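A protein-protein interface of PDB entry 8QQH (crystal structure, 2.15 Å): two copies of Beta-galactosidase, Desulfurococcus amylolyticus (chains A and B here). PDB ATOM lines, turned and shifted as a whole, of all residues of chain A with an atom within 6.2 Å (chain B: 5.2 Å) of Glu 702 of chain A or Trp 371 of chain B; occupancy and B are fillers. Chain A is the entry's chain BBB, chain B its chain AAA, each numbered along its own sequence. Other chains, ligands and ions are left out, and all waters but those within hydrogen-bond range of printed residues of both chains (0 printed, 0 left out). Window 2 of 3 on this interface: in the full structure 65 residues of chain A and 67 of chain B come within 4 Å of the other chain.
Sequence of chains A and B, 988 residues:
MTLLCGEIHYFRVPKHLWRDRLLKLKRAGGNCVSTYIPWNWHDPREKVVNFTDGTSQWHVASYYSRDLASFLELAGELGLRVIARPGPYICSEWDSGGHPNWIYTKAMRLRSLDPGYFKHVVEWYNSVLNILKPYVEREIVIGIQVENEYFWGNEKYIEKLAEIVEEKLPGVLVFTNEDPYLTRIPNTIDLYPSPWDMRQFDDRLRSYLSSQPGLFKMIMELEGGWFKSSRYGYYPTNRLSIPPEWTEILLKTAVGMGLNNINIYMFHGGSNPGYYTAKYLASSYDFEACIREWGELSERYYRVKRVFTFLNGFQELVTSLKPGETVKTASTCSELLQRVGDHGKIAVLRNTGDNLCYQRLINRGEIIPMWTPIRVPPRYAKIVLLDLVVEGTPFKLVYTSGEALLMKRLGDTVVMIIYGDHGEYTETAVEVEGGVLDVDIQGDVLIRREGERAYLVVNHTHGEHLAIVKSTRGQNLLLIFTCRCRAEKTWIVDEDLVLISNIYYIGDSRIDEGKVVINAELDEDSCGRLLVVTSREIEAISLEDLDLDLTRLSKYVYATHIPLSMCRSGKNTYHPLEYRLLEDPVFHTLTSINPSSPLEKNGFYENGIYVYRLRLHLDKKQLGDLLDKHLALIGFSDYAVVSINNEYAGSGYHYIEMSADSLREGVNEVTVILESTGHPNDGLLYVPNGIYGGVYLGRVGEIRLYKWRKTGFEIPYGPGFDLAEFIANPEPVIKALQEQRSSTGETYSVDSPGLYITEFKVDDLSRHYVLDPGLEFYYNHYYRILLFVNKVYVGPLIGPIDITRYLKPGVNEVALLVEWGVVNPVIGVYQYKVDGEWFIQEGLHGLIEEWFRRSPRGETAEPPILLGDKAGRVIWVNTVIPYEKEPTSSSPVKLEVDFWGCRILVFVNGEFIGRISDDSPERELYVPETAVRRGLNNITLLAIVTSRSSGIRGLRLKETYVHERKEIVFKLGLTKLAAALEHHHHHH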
ATOM      1  N   ARG A 699      -9.616 -11.194  14.582  1.00  0.00           N
ATOM      2  CA  ARG A 699     -10.087 -12.323  15.420  1.00  0.00           C
ATOM      3  C   ARG A 699     -11.176 -11.735  16.318  1.00  0.00           C
ATOM      4  O   ARG A 699     -10.922 -10.708  16.969  1.00  0.00           O
ATOM      5  CB  ARG A 699      -8.967 -13.043  16.186  1.00  0.00           C
ATOM      6  CG  ARG A 699      -9.403 -14.376  16.795  1.00  0.00           C
ATOM      7  CD  ARG A 699      -8.295 -15.284  17.315  1.00  0.00           C
ATOM      8  NE  ARG A 699      -7.025 -14.570  17.458  1.00  0.00           N
ATOM      9  CZ  ARG A 699      -6.690 -13.727  18.450  1.00  0.00           C
ATOM     10  NH1 ARG A 699      -7.525 -13.471  19.445  1.00  0.00           N
ATOM     11  NH2 ARG A 699      -5.505 -13.133  18.439  1.00  0.00           N
ATOM     12  N   VAL A 700     -12.366 -12.323  16.257  1.00  0.00           N
ATOM     13  CA  VAL A 700     -13.597 -11.819  16.925  1.00  0.00           C
ATOM     14  C   VAL A 700     -13.931 -12.793  18.056  1.00  0.00           C
ATOM     15  O   VAL A 700     -14.581 -12.386  19.032  1.00  0.00           O
ATOM     16  CB  VAL A 700     -14.717 -11.667  15.881  1.00  0.00           C
ATOM     17  CG1 VAL A 700     -16.104 -11.587  16.504  1.00  0.00           C
ATOM     18  CG2 VAL A 700     -14.445 -10.459  14.992  1.00  0.00           C
ATOM     19  N   GLY A 701     -13.453 -14.029  17.946  1.00  0.00           N
ATOM     20  CA  GLY A 701     -13.413 -14.956  19.085  1.00  0.00           C
ATOM     21  C   GLY A 701     -12.896 -16.316  18.681  1.00  0.00           C
ATOM     22  O   GLY A 701     -12.164 -16.431  17.671  1.00  0.00           O
ATOM     23  N   GLU A 702     -13.288 -17.316  19.452  1.00  0.00           N
ATOM     24  CA  GLU A 702     -12.896 -18.716  19.234  1.00  0.00           C
ATOM     25  C   GLU A 702     -13.932 -19.593  19.914  1.00  0.00           C
ATOM     26  O   GLU A 702     -14.556 -19.142  20.883  1.00  0.00           O
ATOM     27  CB  GLU A 702     -11.511 -18.971  19.819  1.00  0.00           C
ATOM     28  CG  GLU A 702     -11.449 -18.683  21.307  1.00  0.00           C
ATOM     29  CD  GLU A 702     -10.045 -18.459  21.830  1.00  0.00           C
ATOM     30  OE1 GLU A 702      -9.272 -17.721  21.164  1.00  0.00           O
ATOM     31  OE2 GLU A 702      -9.729 -19.029  22.895  1.00  0.00           O
ATOM     32  N   ILE A 703     -14.085 -20.801  19.396  1.00  0.00           N
ATOM     33  CA  ILE A 703     -14.973 -21.849  19.956  1.00  0.00           C
ATOM     34  C   ILE A 703     -14.090 -23.072  20.230  1.00  0.00           C
ATOM     35  O   ILE A 703     -13.530 -23.648  19.268  1.00  0.00           O
ATOM     36  CB  ILE A 703     -16.138 -22.104  18.981  1.00  0.00           C
ATOM     37  CG1 ILE A 703     -16.905 -20.808  18.683  1.00  0.00           C
ATOM     38  CG2 ILE A 703     -17.048 -23.202  19.505  1.00  0.00           C
ATOM     39  CD1 ILE A 703     -17.739 -20.872  17.435  1.00  0.00           C
ATOM     40  N   ARG A 704     -13.901 -23.377  21.510  1.00  0.00           N
ATOM     41  CA  ARG A 704     -13.097 -24.518  21.992  1.00  0.00           C
ATOM     42  C   ARG A 704     -14.016 -25.734  22.001  1.00  0.00           C
ATOM     43  O   ARG A 704     -15.045 -25.660  22.668  1.00  0.00           O
ATOM     44  CB  ARG A 704     -12.532 -24.214  23.381  1.00  0.00           C
ATOM     45  CG  ARG A 704     -11.340 -23.272  23.364  1.00  0.00           C
ATOM     46  CD  ARG A 704     -10.445 -23.408  24.582  1.00  0.00           C
ATOM     47  NE  ARG A 704      -9.627 -22.208  24.704  1.00  0.00           N
ATOM     48  CZ  ARG A 704     -10.026 -21.051  25.241  1.00  0.00           C
ATOM     49  NH1 ARG A 704     -11.242 -20.918  25.743  1.00  0.00           N
ATOM     50  NH2 ARG A 704      -9.196 -20.025  25.282  1.00  0.00           N
ATOM     51  N   LEU A 775      -1.648 -28.227  17.778  1.00  0.00           N
ATOM     52  CA  LEU A 775      -0.237 -28.676  17.829  1.00  0.00           C
ATOM     53  C   LEU A 775      -0.147 -30.213  17.789  1.00  0.00           C
ATOM     54  O   LEU A 775       0.738 -30.714  17.112  1.00  0.00           O
ATOM     55  CB  LEU A 775       0.388 -28.116  19.116  1.00  0.00           C
ATOM     56  CG  LEU A 775       1.823 -28.560  19.391  1.00  0.00           C
ATOM     57  CD1 LEU A 775       2.706 -28.252  18.188  1.00  0.00           C
ATOM     58  CD2 LEU A 775       2.348 -27.887  20.643  1.00  0.00           C
ATOM     59  N   ASN A 824      -6.675 -31.920  18.886  1.00  0.00           N
ATOM     60  CA  ASN A 824      -7.330 -31.010  19.854  1.00  0.00           C
ATOM     61  C   ASN A 824      -7.850 -29.796  19.082  1.00  0.00           C
ATOM     62  O   ASN A 824      -7.235 -28.729  19.072  1.00  0.00           O
ATOM     63  CB  ASN A 824      -6.399 -30.657  21.013  1.00  0.00           C
ATOM     64  CG  ASN A 824      -7.162 -29.997  22.139  1.00  0.00           C
ATOM     65  OD1 ASN A 824      -8.074 -30.590  22.706  1.00  0.00           O
ATOM     66  ND2 ASN A 824      -6.811 -28.763  22.453  1.00  0.00           N
ATOM     67  N   VAL A 826      -9.827 -26.460  17.673  1.00  0.00           N
ATOM     68  CA  VAL A 826     -10.377 -25.170  18.156  1.00  0.00           C
ATOM     69  C   VAL A 826     -10.810 -24.375  16.916  1.00  0.00           C
ATOM     70  O   VAL A 826     -10.124 -24.473  15.883  1.00  0.00           O
ATOM     71  CB  VAL A 826      -9.359 -24.434  19.048  1.00  0.00           C
ATOM     72  CG1 VAL A 826      -8.059 -24.122  18.330  1.00  0.00           C
ATOM     73  CG2 VAL A 826      -9.947 -23.163  19.636  1.00  0.00           C
ATOM     74  N   ILE A 827     -11.910 -23.619  16.997  1.00  0.00           N
ATOM     75  CA  ILE A 827     -12.366 -22.784  15.848  1.00  0.00           C
ATOM     76  C   ILE A 827     -12.010 -21.323  16.117  1.00  0.00           C
ATOM     77  O   ILE A 827     -12.440 -20.795  17.150  1.00  0.00           O
ATOM     78  CB  ILE A 827     -13.870 -22.995  15.587  1.00  0.00           C
ATOM     79  CG1 ILE A 827     -14.153 -24.456  15.202  1.00  0.00           C
ATOM     80  CG2 ILE A 827     -14.368 -22.005  14.532  1.00  0.00           C
ATOM     81  CD1 ILE A 827     -15.494 -24.964  15.683  1.00  0.00           C
ATOM     82  N   GLY A 828     -11.222 -20.715  15.226  1.00  0.00           N
ATOM     83  CA  GLY A 828     -10.996 -19.261  15.199  1.00  0.00           C
ATOM     84  C   GLY A 828     -12.119 -18.580  14.418  1.00  0.00           C
ATOM     85  O   GLY A 828     -12.510 -19.125  13.353  1.00  0.00           O
ATOM     86  N   VAL A 829     -12.655 -17.467  14.937  1.00  0.00           N
ATOM     87  CA  VAL A 829     -13.714 -16.660  14.250  1.00  0.00           C
ATOM     88  C   VAL A 829     -13.117 -15.322  13.806  1.00  0.00           C
ATOM     89  O   VAL A 829     -12.621 -14.574  14.676  1.00  0.00           O
ATOM     90  CB  VAL A 829     -14.945 -16.455  15.145  1.00  0.00           C
ATOM     91  CG1 VAL A 829     -16.128 -15.952  14.326  1.00  0.00           C
ATOM     92  CG2 VAL A 829     -15.299 -17.730  15.898  1.00  0.00           C
ATOM     93  N   ARG B 360      -3.301 -32.185  29.304  1.00  0.00           N
ATOM     94  CA  ARG B 360      -4.066 -31.013  29.813  1.00  0.00           C
ATOM     95  C   ARG B 360      -4.535 -31.372  31.213  1.00  0.00           C
ATOM     96  O   ARG B 360      -4.600 -32.563  31.500  1.00  0.00           O
ATOM     97  CB  ARG B 360      -5.222 -30.671  28.864  1.00  0.00           C
ATOM     98  CG  ARG B 360      -4.747 -30.020  27.575  1.00  0.00           C
ATOM     99  CD  ARG B 360      -5.810 -29.815  26.516  1.00  0.00           C
ATOM    100  NE  ARG B 360      -5.218 -29.388  25.245  1.00  0.00           N
ATOM    101  CZ  ARG B 360      -4.921 -28.127  24.897  1.00  0.00           C
ATOM    102  NH1 ARG B 360      -5.149 -27.110  25.718  1.00  0.00           N
ATOM    103  NH2 ARG B 360      -4.390 -27.894  23.709  1.00  0.00           N
ATOM    104  N   PRO B 369      -3.579 -26.008  29.798  1.00  0.00           N
ATOM    105  CA  PRO B 369      -3.683 -24.597  29.385  1.00  0.00           C
ATOM    106  C   PRO B 369      -4.755 -24.366  28.294  1.00  0.00           C
ATOM    107  O   PRO B 369      -5.386 -25.324  27.891  1.00  0.00           O
ATOM    108  CB  PRO B 369      -2.291 -24.263  28.817  1.00  0.00           C
ATOM    109  CG  PRO B 369      -1.426 -25.479  29.136  1.00  0.00           C
ATOM    110  CD  PRO B 369      -2.396 -26.634  29.197  1.00  0.00           C
ATOM    111  N   MET B 370      -4.910 -23.133  27.798  1.00  0.00           N
ATOM    112  CA  MET B 370      -6.031 -22.729  26.890  1.00  0.00           C
ATOM    113  C   MET B 370      -5.714 -23.004  25.409  1.00  0.00           C
ATOM    114  O   MET B 370      -6.586 -23.562  24.726  1.00  0.00           O
ATOM    115  CB  MET B 370      -6.368 -21.241  27.027  1.00  0.00           C
ATOM    116  CG  MET B 370      -6.484 -20.745  28.462  1.00  0.00           C
ATOM    117  SD  MET B 370      -8.020 -21.214  29.272  1.00  0.00           S
ATOM    118  CE  MET B 370      -8.144 -19.868  30.449  1.00  0.00           C
ATOM    119  N   TRP B 371      -4.562 -22.571  24.894  1.00  0.00           N
ATOM    120  CA  TRP B 371      -4.226 -22.676  23.441  1.00  0.00           C
ATOM    121  C   TRP B 371      -3.235 -23.801  23.163  1.00  0.00           C
ATOM    122  O   TRP B 371      -3.097 -24.123  22.001  1.00  0.00           O
ATOM    123  CB  TRP B 371      -3.715 -21.338  22.880  1.00  0.00           C
ATOM    124  CG  TRP B 371      -4.803 -20.334  23.030  1.00  0.00           C
ATOM    125  CD1 TRP B 371      -5.973 -20.298  22.329  1.00  0.00           C
ATOM    126  CD2 TRP B 371      -4.923 -19.375  24.090  1.00  0.00           C
ATOM    127  NE1 TRP B 371      -6.788 -19.334  22.848  1.00  0.00           N
ATOM    128  CE2 TRP B 371      -6.177 -18.750  23.928  1.00  0.00           C
ATOM    129  CE3 TRP B 371      -4.086 -18.972  25.139  1.00  0.00           C
ATOM    130  CZ2 TRP B 371      -6.605 -17.719  24.767  1.00  0.00           C
ATOM    131  CZ3 TRP B 371      -4.518 -17.965  25.974  1.00  0.00           C
ATOM    132  CH2 TRP B 371      -5.758 -17.345  25.787  1.00  0.00           C
ATOM    133  N   THR B 372      -2.565 -24.334  24.184  1.00  0.00           N
ATOM    134  CA  THR B 372      -1.380 -25.207  24.034  1.00  0.00           C
ATOM    135  C   THR B 372      -1.537 -26.395  24.971  1.00  0.00           C
ATOM    136  O   THR B 372      -1.991 -26.230  26.097  1.00  0.00           O
ATOM    137  CB  THR B 372      -0.092 -24.426  24.321  1.00  0.00           C
ATOM    138  OG1 THR B 372      -0.330 -23.021  24.263  1.00  0.00           O
ATOM    139  CG2 THR B 372       1.001 -24.746  23.331  1.00  0.00           C
ATOM    140  N   PRO B 373      -1.165 -27.621  24.543  1.00  0.00           N
ATOM    141  CA  PRO B 373      -1.077 -28.753  25.461  1.00  0.00           C
ATOM    142  C   PRO B 373       0.216 -28.664  26.282  1.00  0.00           C
ATOM    143  O   PRO B 373       1.151 -27.993  25.845  1.00  0.00           O
ATOM    144  CB  PRO B 373      -1.070 -29.953  24.512  1.00  0.00           C
ATOM    145  CG  PRO B 373      -0.317 -29.422  23.303  1.00  0.00           C
ATOM    146  CD  PRO B 373      -0.784 -27.987  23.170  1.00  0.00           C
ATOM    147  N   GLU B 427       2.790 -22.306  27.777  1.00  0.00           N
ATOM    148  CA  GLU B 427       1.758 -21.280  28.037  1.00  0.00           C
ATOM    149  C   GLU B 427       1.809 -20.989  29.524  1.00  0.00           C
ATOM    150  O   GLU B 427       1.761 -21.951  30.304  1.00  0.00           O
ATOM    151  CB  GLU B 427       0.404 -21.794  27.567  1.00  0.00           C
ATOM    152  CG  GLU B 427      -0.690 -20.745  27.556  1.00  0.00           C
ATOM    153  CD  GLU B 427      -2.045 -21.320  27.174  1.00  0.00           C
ATOM    154  OE1 GLU B 427      -2.970 -21.257  28.023  1.00  0.00           O
ATOM    155  OE2 GLU B 427      -2.166 -21.875  26.054  1.00  0.00           O
ATOM    156  N   ARG B 448      -1.625 -12.699  25.154  1.00  0.00           N
ATOM    157  CA  ARG B 448      -3.099 -12.519  25.144  1.00  0.00           C
ATOM    158  C   ARG B 448      -3.458 -11.899  26.490  1.00  0.00           C
ATOM    159  O   ARG B 448      -3.194 -12.554  27.518  1.00  0.00           O
ATOM    160  CB  ARG B 448      -3.799 -13.860  24.912  1.00  0.00           C
ATOM    161  CG  ARG B 448      -5.310 -13.793  24.733  1.00  0.00           C
ATOM    162  CD  ARG B 448      -5.769 -13.750  23.280  1.00  0.00           C
ATOM    163  NE  ARG B 448      -5.138 -14.768  22.431  1.00  0.00           N
ATOM    164  CZ  ARG B 448      -5.763 -15.741  21.760  1.00  0.00           C
ATOM    165  NH1 ARG B 448      -7.079 -15.870  21.815  1.00  0.00           N
ATOM    166  NH2 ARG B 448      -5.053 -16.591  21.029  1.00  0.00           N
ATOM    167  N   GLU B 450      -6.682 -10.772  28.757  1.00  0.00           N
ATOM    168  CA  GLU B 450      -8.140 -11.027  28.905  1.00  0.00           C
ATOM    169  C   GLU B 450      -8.669 -10.204  30.083  1.00  0.00           C
ATOM    170  O   GLU B 450      -9.354  -9.191  29.818  1.00  0.00           O
ATOM    171  CB  GLU B 450      -8.433 -12.522  29.049  1.00  0.00           C
ATOM    172  CG  GLU B 450      -8.429 -13.256  27.713  1.00  0.00           C
ATOM    173  CD  GLU B 450      -9.483 -14.341  27.541  1.00  0.00           C
ATOM    174  OE1 GLU B 450     -10.501 -14.293  28.261  1.00  0.00           O
ATOM    175  OE2 GLU B 450      -9.292 -15.225  26.672  1.00  0.00           O
ATOM    176  N   TYR B 455      -1.777 -13.965  29.361  1.00  0.00           N
ATOM    177  CA  TYR B 455      -1.347 -15.275  28.820  1.00  0.00           C
ATOM    178  C   TYR B 455      -0.090 -15.056  27.956  1.00  0.00           C
ATOM    179  O   TYR B 455      -0.104 -14.191  27.051  1.00  0.00           O
ATOM    180  CB  TYR B 455      -2.508 -15.962  28.109  1.00  0.00           C
ATOM    181  CG  TYR B 455      -3.710 -16.256  28.982  1.00  0.00           C
ATOM    182  CD1 TYR B 455      -4.672 -15.281  29.218  1.00  0.00           C
ATOM    183  CD2 TYR B 455      -3.918 -17.511  29.541  1.00  0.00           C
ATOM    184  CE1 TYR B 455      -5.799 -15.536  29.983  1.00  0.00           C
ATOM    185  CE2 TYR B 455      -5.032 -17.778  30.325  1.00  0.00           C
ATOM    186  CZ  TYR B 455      -5.986 -16.787  30.536  1.00  0.00           C
ATOM    187  OH  TYR B 455      -7.093 -17.012  31.304  1.00  0.00           O
ATOM    188  N   VAL B 457       2.589 -17.135  25.640  1.00  0.00           N
ATOM    189  CA  VAL B 457       2.888 -18.332  24.810  1.00  0.00           C
ATOM    190  C   VAL B 457       4.304 -18.169  24.245  1.00  0.00           C
ATOM    191  O   VAL B 457       4.565 -17.143  23.598  1.00  0.00           O
ATOM    192  CB  VAL B 457       1.856 -18.559  23.695  1.00  0.00           C
ATOM    193  CG1 VAL B 457       2.244 -19.766  22.849  1.00  0.00           C
ATOM    194  CG2 VAL B 457       0.451 -18.753  24.248  1.00  0.00           C
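ND2 of Asn 824 of chain A lies close to NH2 of Arg 360 of chain B (2.9 Å). O of Met 370 of chain B sits at hydrogen-bond distance from NE of Arg 704 of chain A. The indole nitrogen (NE1) of Trp 371 of chain B lies within hydrogen-bond range of the side-chain carboxylate (OE2) of Glu 702 of chain A (3.0 Å). The side-chain carboxylate (OE1) of Glu 702 of chain A lies within salt-bridge range of the guanidinium group (NH1) of Arg 448 of chain B (2.9 Å). The guanidinium group (NH1) of Arg 699 of chain A sits close to the guanidinium group (NH1) of Arg 448 of chain B (3.4 Å). The guanidinium group (NH2) of Arg 704 of chain A sits close to the indole nitrogen (NE1) of Trp 371 of chain B (3.5 Å).
The guanidinium group (NH1) of Arg 360 of chain B sits at hydrogen-bond distance from the backbone carbonyl oxygen (O) of Pro 369 of chain B (2.8 Å). NH1 of Arg 360 of chain B lies within hydrogen-bond range of O of Thr 372 of chain B, at 3.3 Å. The backbone NH (N) of Met 370 of chain B lies within hydrogen-bond range of the side-chain carboxylate (OE1) of Glu 427 of chain B, 2.7 Å away. The side-chain carboxylate of Glu 427 of chain B sits at hydrogen-bond distance from the backbone NH of Trp 371 of chain B, at 2.8 Å. The backbone NH (N) of Tyr 455 of chain B is in hydrogen-bond range of the backbone carbonyl oxygen (O) of Arg 448 of chain B (2.7 Å). The side-chain carboxylate (OE2) of Glu 702 of chain A is in salt-bridge range of the guanidinium group (NH2) of Arg 704 of chain A (2.6 Å).
Of the printed residues of chain B, Arg 699 of chain A touches Arg 448. Glu 702 of chain A touches just these residues of chain B: Trp 371 (3.0 Å) and Arg 448 (2.9 Å). Gly 828 of chain A touches none of the printed residues of chain B. Val 829 of chain A touches none of the printed residues of chain B. Printed residues of chain A within 4 Å of Arg 360 of chain B: Asn 824. Of the printed residues of chain A, Trp 371 of chain B touches Glu 702 (3.0 Å) and Arg 704 (3.5 Å). The nearest printed residue of chain A that does not touch Arg 360 of chain B is Leu 775 of chain A (6.5 Å).
Of the 12 printed residues of chain A, 4 touch a printed residue of chain B.
No position is printed for both chains. Of the 6 pairs that touch across the chains among the printed residues, none has its exchanged pair printed and touching as well.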
